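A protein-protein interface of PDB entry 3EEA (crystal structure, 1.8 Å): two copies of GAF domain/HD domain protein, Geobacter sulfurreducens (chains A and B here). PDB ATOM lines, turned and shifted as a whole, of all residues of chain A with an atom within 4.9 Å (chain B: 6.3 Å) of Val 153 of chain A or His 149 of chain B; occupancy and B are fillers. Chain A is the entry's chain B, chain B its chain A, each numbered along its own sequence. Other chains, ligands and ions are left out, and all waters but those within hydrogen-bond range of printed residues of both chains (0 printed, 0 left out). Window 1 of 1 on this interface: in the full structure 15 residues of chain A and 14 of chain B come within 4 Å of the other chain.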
ATOM      1  N   THR A  12     -12.243 -20.264 -14.145  1.00  0.00           N
ATOM      2  CA  THR A  12     -13.189 -19.997 -13.068  1.00  0.00           C
ATOM      3  C   THR A  12     -14.469 -19.425 -13.667  1.00  0.00           C
ATOM      4  O   THR A  12     -14.572 -19.218 -14.894  1.00  0.00           O
ATOM      5  CB  THR A  12     -12.552 -19.061 -11.987  1.00  0.00           C
ATOM      6  OG1 THR A  12     -13.420 -18.952 -10.847  1.00  0.00           O
ATOM      7  CG2 THR A  12     -12.309 -17.631 -12.536  1.00  0.00           C
ATOM      8  N   VAL A  17     -16.268 -18.616  -7.959  1.00  0.00           N
ATOM      9  CA  VAL A  17     -15.719 -17.572  -7.063  1.00  0.00           C
ATOM     10  C   VAL A  17     -16.519 -17.462  -5.781  1.00  0.00           C
ATOM     11  O   VAL A  17     -15.932 -17.403  -4.680  1.00  0.00           O
ATOM     12  CB  VAL A  17     -15.618 -16.171  -7.762  1.00  0.00           C
ATOM     13  CG1 VAL A  17     -15.213 -15.060  -6.733  1.00  0.00           C
ATOM     14  CG2 VAL A  17     -14.582 -16.268  -8.902  1.00  0.00           C
ATOM     15  N   ASP A  20     -15.772 -20.443  -3.577  1.00  0.00           N
ATOM     16  CA  ASP A  20     -14.458 -20.214  -2.996  1.00  0.00           C
ATOM     17  C   ASP A  20     -14.508 -19.191  -1.847  1.00  0.00           C
ATOM     18  O   ASP A  20     -13.876 -19.384  -0.791  1.00  0.00           O
ATOM     19  CB  ASP A  20     -13.462 -19.727  -4.042  1.00  0.00           C
ATOM     20  CG  ASP A  20     -13.131 -20.763  -5.130  1.00  0.00           C
ATOM     21  OD1 ASP A  20     -13.461 -21.985  -4.999  1.00  0.00           O
ATOM     22  OD2 ASP A  20     -12.525 -20.296  -6.143  1.00  0.00           O
ATOM     23  N   HIS A 149     -11.637  -8.910  -2.778  1.00  0.00           N
ATOM     24  CA  HIS A 149     -11.121  -9.733  -3.845  1.00  0.00           C
ATOM     25  C   HIS A 149     -12.260 -10.314  -4.696  1.00  0.00           C
ATOM     26  O   HIS A 149     -12.227 -10.246  -5.937  1.00  0.00           O
ATOM     27  CB  HIS A 149     -10.263 -10.865  -3.281  1.00  0.00           C
ATOM     28  CG  HIS A 149      -9.753 -11.828  -4.322  1.00  0.00           C
ATOM     29  ND1 HIS A 149     -10.456 -12.957  -4.721  1.00  0.00           N
ATOM     30  CD2 HIS A 149      -8.597 -11.838  -5.024  1.00  0.00           C
ATOM     31  CE1 HIS A 149      -9.737 -13.623  -5.612  1.00  0.00           C
ATOM     32  NE2 HIS A 149      -8.599 -12.973  -5.801  1.00  0.00           N
ATOM     33  N   ALA A 150     -13.214 -10.986  -4.021  1.00  0.00           N
ATOM     34  CA  ALA A 150     -14.276 -11.623  -4.743  1.00  0.00           C
ATOM     35  C   ALA A 150     -15.034 -10.599  -5.559  1.00  0.00           C
ATOM     36  O   ALA A 150     -15.360 -10.862  -6.682  1.00  0.00           O
ATOM     37  CB  ALA A 150     -15.212 -12.403  -3.811  1.00  0.00           C
ATOM     38  N   ALA A 151     -15.358  -9.440  -4.967  1.00  0.00           N
ATOM     39  CA  ALA A 151     -16.109  -8.400  -5.660  1.00  0.00           C
ATOM     40  C   ALA A 151     -15.509  -7.974  -6.950  1.00  0.00           C
ATOM     41  O   ALA A 151     -16.229  -7.872  -7.933  1.00  0.00           O
ATOM     42  CB  ALA A 151     -16.337  -7.209  -4.734  1.00  0.00           C
ATOM     43  N   LEU A 152     -14.192  -7.767  -6.969  1.00  0.00           N
ATOM     44  CA  LEU A 152     -13.541  -7.259  -8.176  1.00  0.00           C
ATOM     45  C   LEU A 152     -13.569  -8.331  -9.282  1.00  0.00           C
ATOM     46  O   LEU A 152     -13.894  -8.049 -10.443  1.00  0.00           O
ATOM     47  CB  LEU A 152     -12.117  -6.836  -7.885  1.00  0.00           C
ATOM     48  CG  LEU A 152     -11.313  -6.392  -9.127  1.00  0.00           C
ATOM     49  CD1 LEU A 152     -11.930  -5.098  -9.736  1.00  0.00           C
ATOM     50  CD2 LEU A 152      -9.844  -6.201  -8.772  1.00  0.00           C
ATOM     51  N   VAL A 153     -13.307  -9.580  -8.907  1.00  0.00           N
ATOM     52  CA  VAL A 153     -13.309 -10.668  -9.907  1.00  0.00           C
ATOM     53  C   VAL A 153     -14.696 -10.887 -10.460  1.00  0.00           C
ATOM     54  O   VAL A 153     -14.893 -11.000 -11.669  1.00  0.00           O
ATOM     55  CB  VAL A 153     -12.717 -11.977  -9.374  1.00  0.00           C
ATOM     56  CG1 VAL A 153     -12.453 -12.938 -10.559  1.00  0.00           C
ATOM     57  CG2 VAL A 153     -11.440 -11.666  -8.662  1.00  0.00           C
ATOM     58  N   VAL A 154     -15.668 -10.907  -9.577  1.00  0.00           N
ATOM     59  CA  VAL A 154     -17.062 -11.097  -9.972  1.00  0.00           C
ATOM     60  C   VAL A 154     -17.522  -9.973 -10.875  1.00  0.00           C
ATOM     61  O   VAL A 154     -18.182 -10.224 -11.881  1.00  0.00           O
ATOM     62  CB  VAL A 154     -17.981 -11.261  -8.744  1.00  0.00           C
ATOM     63  CG1 VAL A 154     -19.486 -11.119  -9.150  1.00  0.00           C
ATOM     64  CG2 VAL A 154     -17.712 -12.607  -8.122  1.00  0.00           C
ATOM     65  N   SER A 155     -17.163  -8.745 -10.534  1.00  0.00           N
ATOM     66  CA  SER A 155     -17.567  -7.626 -11.376  1.00  0.00           C
ATOM     67  C   SER A 155     -16.971  -7.699 -12.756  1.00  0.00           C
ATOM     68  O   SER A 155     -17.664  -7.347 -13.751  1.00  0.00           O
ATOM     69  CB  SER A 155     -17.301  -6.275 -10.714  1.00  0.00           C
ATOM     70  OG  SER A 155     -15.905  -6.009 -10.547  1.00  0.00           O
ATOM     71  N   HIS A 156     -15.700  -8.134 -12.858  1.00  0.00           N
ATOM     72  CA  HIS A 156     -15.061  -8.314 -14.151  1.00  0.00           C
ATOM     73  C   HIS A 156     -15.777  -9.413 -14.962  1.00  0.00           C
ATOM     74  O   HIS A 156     -16.011  -9.265 -16.143  1.00  0.00           O
ATOM     75  CB  HIS A 156     -13.537  -8.599 -14.006  1.00  0.00           C
ATOM     76  CG  HIS A 156     -12.688  -7.375 -13.988  1.00  0.00           C
ATOM     77  ND1 HIS A 156     -11.879  -7.040 -15.044  1.00  0.00           N
ATOM     78  CD2 HIS A 156     -12.530  -6.393 -13.066  1.00  0.00           C
ATOM     79  CE1 HIS A 156     -11.270  -5.898 -14.790  1.00  0.00           C
ATOM     80  NE2 HIS A 156     -11.640  -5.485 -13.593  1.00  0.00           N
ATOM     81  N   MET A 157     -16.092 -10.525 -14.333  1.00  0.00           N
ATOM     82  CA  MET A 157     -16.792 -11.578 -15.029  1.00  0.00           C
ATOM     83  C   MET A 157     -18.185 -11.156 -15.489  1.00  0.00           C
ATOM     84  O   MET A 157     -18.580 -11.407 -16.577  1.00  0.00           O
ATOM     85  CB  MET A 157     -16.857 -12.857 -14.212  1.00  0.00           C
ATOM     86  CG  MET A 157     -15.598 -13.230 -13.607  1.00  0.00           C
ATOM     87  SD  MET A 157     -15.630 -14.743 -12.601  1.00  0.00           S
ATOM     88  CE  MET A 157     -15.008 -15.603 -13.847  1.00  0.00           C
ATOM     89  N   VAL B  17      -3.648  -4.587  -8.712  1.00  0.00           N
ATOM     90  CA  VAL B  17      -4.176  -5.961  -8.722  1.00  0.00           C
ATOM     91  C   VAL B  17      -3.083  -6.927  -8.173  1.00  0.00           C
ATOM     92  O   VAL B  17      -3.356  -7.772  -7.301  1.00  0.00           O
ATOM     93  CB  VAL B  17      -4.677  -6.379 -10.112  1.00  0.00           C
ATOM     94  CG1 VAL B  17      -5.128  -7.866 -10.138  1.00  0.00           C
ATOM     95  CG2 VAL B  17      -5.898  -5.468 -10.575  1.00  0.00           C
ATOM     96  N   ARG B 144      -3.590 -21.483  -6.510  1.00  0.00           N
ATOM     97  CA  ARG B 144      -3.966 -21.584  -7.915  1.00  0.00           C
ATOM     98  C   ARG B 144      -5.280 -20.830  -8.224  1.00  0.00           C
ATOM     99  O   ARG B 144      -5.414 -20.133  -9.255  1.00  0.00           O
ATOM    100  CB  ARG B 144      -4.097 -23.081  -8.304  1.00  0.00           C
ATOM    101  CG  ARG B 144      -2.760 -23.713  -8.385  1.00  0.00           C
ATOM    102  CD  ARG B 144      -2.844 -25.235  -8.627  1.00  0.00           C
ATOM    103  NE  ARG B 144      -3.553 -25.473  -9.879  1.00  0.00           N
ATOM    104  CZ  ARG B 144      -3.912 -26.684 -10.317  1.00  0.00           C
ATOM    105  NH1 ARG B 144      -3.698 -27.762  -9.588  1.00  0.00           N
ATOM    106  NH2 ARG B 144      -4.506 -26.771 -11.478  1.00  0.00           N
ATOM    107  N   ASP B 145      -6.247 -20.955  -7.324  1.00  0.00           N
ATOM    108  CA  ASP B 145      -7.527 -20.247  -7.477  1.00  0.00           C
ATOM    109  C   ASP B 145      -7.337 -18.738  -7.521  1.00  0.00           C
ATOM    110  O   ASP B 145      -7.819 -18.047  -8.458  1.00  0.00           O
ATOM    111  CB  ASP B 145      -8.455 -20.625  -6.340  1.00  0.00           C
ATOM    112  CG  ASP B 145      -9.094 -21.999  -6.522  1.00  0.00           C
ATOM    113  OD1 ASP B 145      -9.262 -22.441  -7.660  1.00  0.00           O
ATOM    114  OD2 ASP B 145      -9.537 -22.571  -5.485  1.00  0.00           O
ATOM    115  N   LEU B 146      -6.617 -18.220  -6.511  1.00  0.00           N
ATOM    116  CA  LEU B 146      -6.462 -16.752  -6.345  1.00  0.00           C
ATOM    117  C   LEU B 146      -5.643 -16.158  -7.514  1.00  0.00           C
ATOM    118  O   LEU B 146      -6.006 -15.153  -8.101  1.00  0.00           O
ATOM    119  CB  LEU B 146      -5.824 -16.429  -5.011  1.00  0.00           C
ATOM    120  CG  LEU B 146      -6.759 -16.629  -3.816  1.00  0.00           C
ATOM    121  CD1 LEU B 146      -6.115 -16.126  -2.526  1.00  0.00           C
ATOM    122  CD2 LEU B 146      -8.094 -15.974  -4.001  1.00  0.00           C
ATOM    123  N   VAL B 147      -4.608 -16.865  -7.936  1.00  0.00           N
ATOM    124  CA  VAL B 147      -3.793 -16.453  -9.059  1.00  0.00           C
ATOM    125  C   VAL B 147      -4.621 -16.483 -10.327  1.00  0.00           C
ATOM    126  O   VAL B 147      -4.498 -15.617 -11.162  1.00  0.00           O
ATOM    127  CB  VAL B 147      -2.508 -17.313  -9.200  1.00  0.00           C
ATOM    128  CG1 VAL B 147      -1.730 -17.059 -10.544  1.00  0.00           C
ATOM    129  CG2 VAL B 147      -1.626 -17.100  -7.982  1.00  0.00           C
ATOM    130  N   SER B 148      -5.498 -17.474 -10.480  1.00  0.00           N
ATOM    131  CA  SER B 148      -6.316 -17.548 -11.662  1.00  0.00           C
ATOM    132  C   SER B 148      -7.303 -16.429 -11.718  1.00  0.00           C
ATOM    133  O   SER B 148      -7.584 -15.912 -12.797  1.00  0.00           O
ATOM    134  CB  SER B 148      -7.021 -18.880 -11.788  1.00  0.00           C
ATOM    135  OG  SER B 148      -6.020 -19.861 -11.932  1.00  0.00           O
ATOM    136  N   HIS B 149      -7.849 -16.028 -10.551  1.00  0.00           N
ATOM    137  CA  HIS B 149      -8.687 -14.865 -10.506  1.00  0.00           C
ATOM    138  C   HIS B 149      -7.976 -13.579 -10.945  1.00  0.00           C
ATOM    139  O   HIS B 149      -8.532 -12.773 -11.726  1.00  0.00           O
ATOM    140  CB  HIS B 149      -9.264 -14.666  -9.111  1.00  0.00           C
ATOM    141  CG  HIS B 149     -10.063 -15.809  -8.616  1.00  0.00           C
ATOM    142  ND1 HIS B 149     -10.357 -15.972  -7.277  1.00  0.00           N
ATOM    143  CD2 HIS B 149     -10.578 -16.884  -9.256  1.00  0.00           C
ATOM    144  CE1 HIS B 149     -11.020 -17.102  -7.121  1.00  0.00           C
ATOM    145  NE2 HIS B 149     -11.181 -17.668  -8.299  1.00  0.00           N
ATOM    146  N   ALA B 150      -6.765 -13.360 -10.397  1.00  0.00           N
ATOM    147  CA  ALA B 150      -5.967 -12.194 -10.706  1.00  0.00           C
ATOM    148  C   ALA B 150      -5.584 -12.190 -12.158  1.00  0.00           C
ATOM    149  O   ALA B 150      -5.628 -11.112 -12.819  1.00  0.00           O
ATOM    150  CB  ALA B 150      -4.664 -12.108  -9.777  1.00  0.00           C
ATOM    151  N   ALA B 151      -5.236 -13.360 -12.720  1.00  0.00           N
ATOM    152  CA  ALA B 151      -4.865 -13.453 -14.110  1.00  0.00           C
ATOM    153  C   ALA B 151      -5.994 -13.004 -15.034  1.00  0.00           C
ATOM    154  O   ALA B 151      -5.748 -12.289 -16.017  1.00  0.00           O
ATOM    155  CB  ALA B 151      -4.402 -14.915 -14.489  1.00  0.00           C
ATOM    156  N   LEU B 152      -7.228 -13.392 -14.731  1.00  0.00           N
ATOM    157  CA  LEU B 152      -8.364 -13.037 -15.567  1.00  0.00           C
ATOM    158  C   LEU B 152      -8.602 -11.510 -15.575  1.00  0.00           C
ATOM    159  O   LEU B 152      -8.818 -10.852 -16.640  1.00  0.00           O
ATOM    160  CB  LEU B 152      -9.588 -13.758 -15.025  1.00  0.00           C
ATOM    161  CG  LEU B 152     -10.925 -13.486 -15.638  1.00  0.00           C
ATOM    162  CD1 LEU B 152     -10.859 -13.773 -17.145  1.00  0.00           C
ATOM    163  CD2 LEU B 152     -11.912 -14.505 -14.892  1.00  0.00           C
ATOM    164  N   VAL B 153      -8.511 -10.943 -14.387  1.00  0.00           N
ATOM    165  CA  VAL B 153      -8.638  -9.497 -14.206  1.00  0.00           C
ATOM    166  C   VAL B 153      -7.553  -8.757 -14.991  1.00  0.00           C
ATOM    167  O   VAL B 153      -7.863  -7.786 -15.727  1.00  0.00           O
ATOM    168  CB  VAL B 153      -8.582  -9.076 -12.718  1.00  0.00           C
ATOM    169  CG1 VAL B 153      -8.585  -7.510 -12.605  1.00  0.00           C
ATOM    170  CG2 VAL B 153      -9.833  -9.613 -11.929  1.00  0.00           C
ATOM    171  N   VAL B 154      -6.309  -9.171 -14.799  1.00  0.00           N
ATOM    172  CA  VAL B 154      -5.129  -8.537 -15.455  1.00  0.00           C
ATOM    173  C   VAL B 154      -5.272  -8.645 -16.958  1.00  0.00           C
ATOM    174  O   VAL B 154      -5.059  -7.667 -17.686  1.00  0.00           O
ATOM    175  CB  VAL B 154      -3.776  -9.124 -14.972  1.00  0.00           C
ATOM    176  CG1 VAL B 154      -2.591  -8.595 -15.881  1.00  0.00           C
ATOM    177  CG2 VAL B 154      -3.533  -8.695 -13.497  1.00  0.00           C
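Printed residues of chain B within 4 Å of Thr 12 of chain A: His 149 and Leu 152. Printed residues of chain B within 4 Å of His 149 of chain A: Leu 146 and His 149. Printed residues of chain B within 4 Å of Val 153 of chain A: His 149 (3.7 Å). Of the printed residues of chain B, His 156 of chain A touches Val 153. His 149 of chain B touches just these residues of chain A: Thr 12 (3.6 Å), Val 17 (3.7 Å), Asp 20 (3.7 Å), His 149 (2.9 Å) and Val 153 (3.7 Å). Printed residues of chain A within 4 Å of Leu 152 of chain B: Thr 12 (3.9 Å) and Met 157 (3.4 Å). The nearest printed residue of chain A that does not touch His 149 of chain B is Ala 150 of chain A (6.4 Å). The nearest printed residue of chain B that does not touch His 156 of chain A is Leu 152 of chain B (5.1 Å).
O of Asp 145 of chain B lies close to NE2 of His 149 of chain B (3.4 Å).
Among the printed residues, merely in contact across the chains: His 149 of chain A with His 149 of chain B, His 149 of chain A with Leu 146 of chain B, Met 157 of chain A with Leu 152 of chain B, Thr 12 of chain A with His 149 of chain B, Asp 20 of chain A with His 149 of chain B, Val 17 of chain A with His 149 of chain B, Val 153 of chain A with His 149 of chain B, His 156 of chain A with Val 153 of chain B, Asp 20 of chain A with Asp 145 of chain B and Thr 12 of chain A with Leu 152 of chain B.
Of the 12 printed residues of chain A, 7 touch a printed residue of chain B. Hydrophobic or aromatic side chains of chain A that line the printed part of chain B: Val 17, His 149, Val 153, His 156 and Met 157. Among the printed residues, 10 pairs touch across the chains. Among the printed residues, no Asp or Glu carboxylate lies within 4 Å of a Lys or Arg side-chain nitrogen of the other chain.
Val 17 of chain A touches His 149 of chain B, but with the chains exchanged His 149 of chain A does not touch Val 17 of chain B (7.0 Å). His 149 of chain A touches its own counterpart, His 149 of chain B. Val 153 of chain A touches His 149 of chain B, but with the chains exchanged His 149 of chain A does not touch Val 153 of chain B (6.5 Å). Of the 10 pairs that touch across the chains among the printed residues, 1 has its exchanged pair printed and touching as well.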
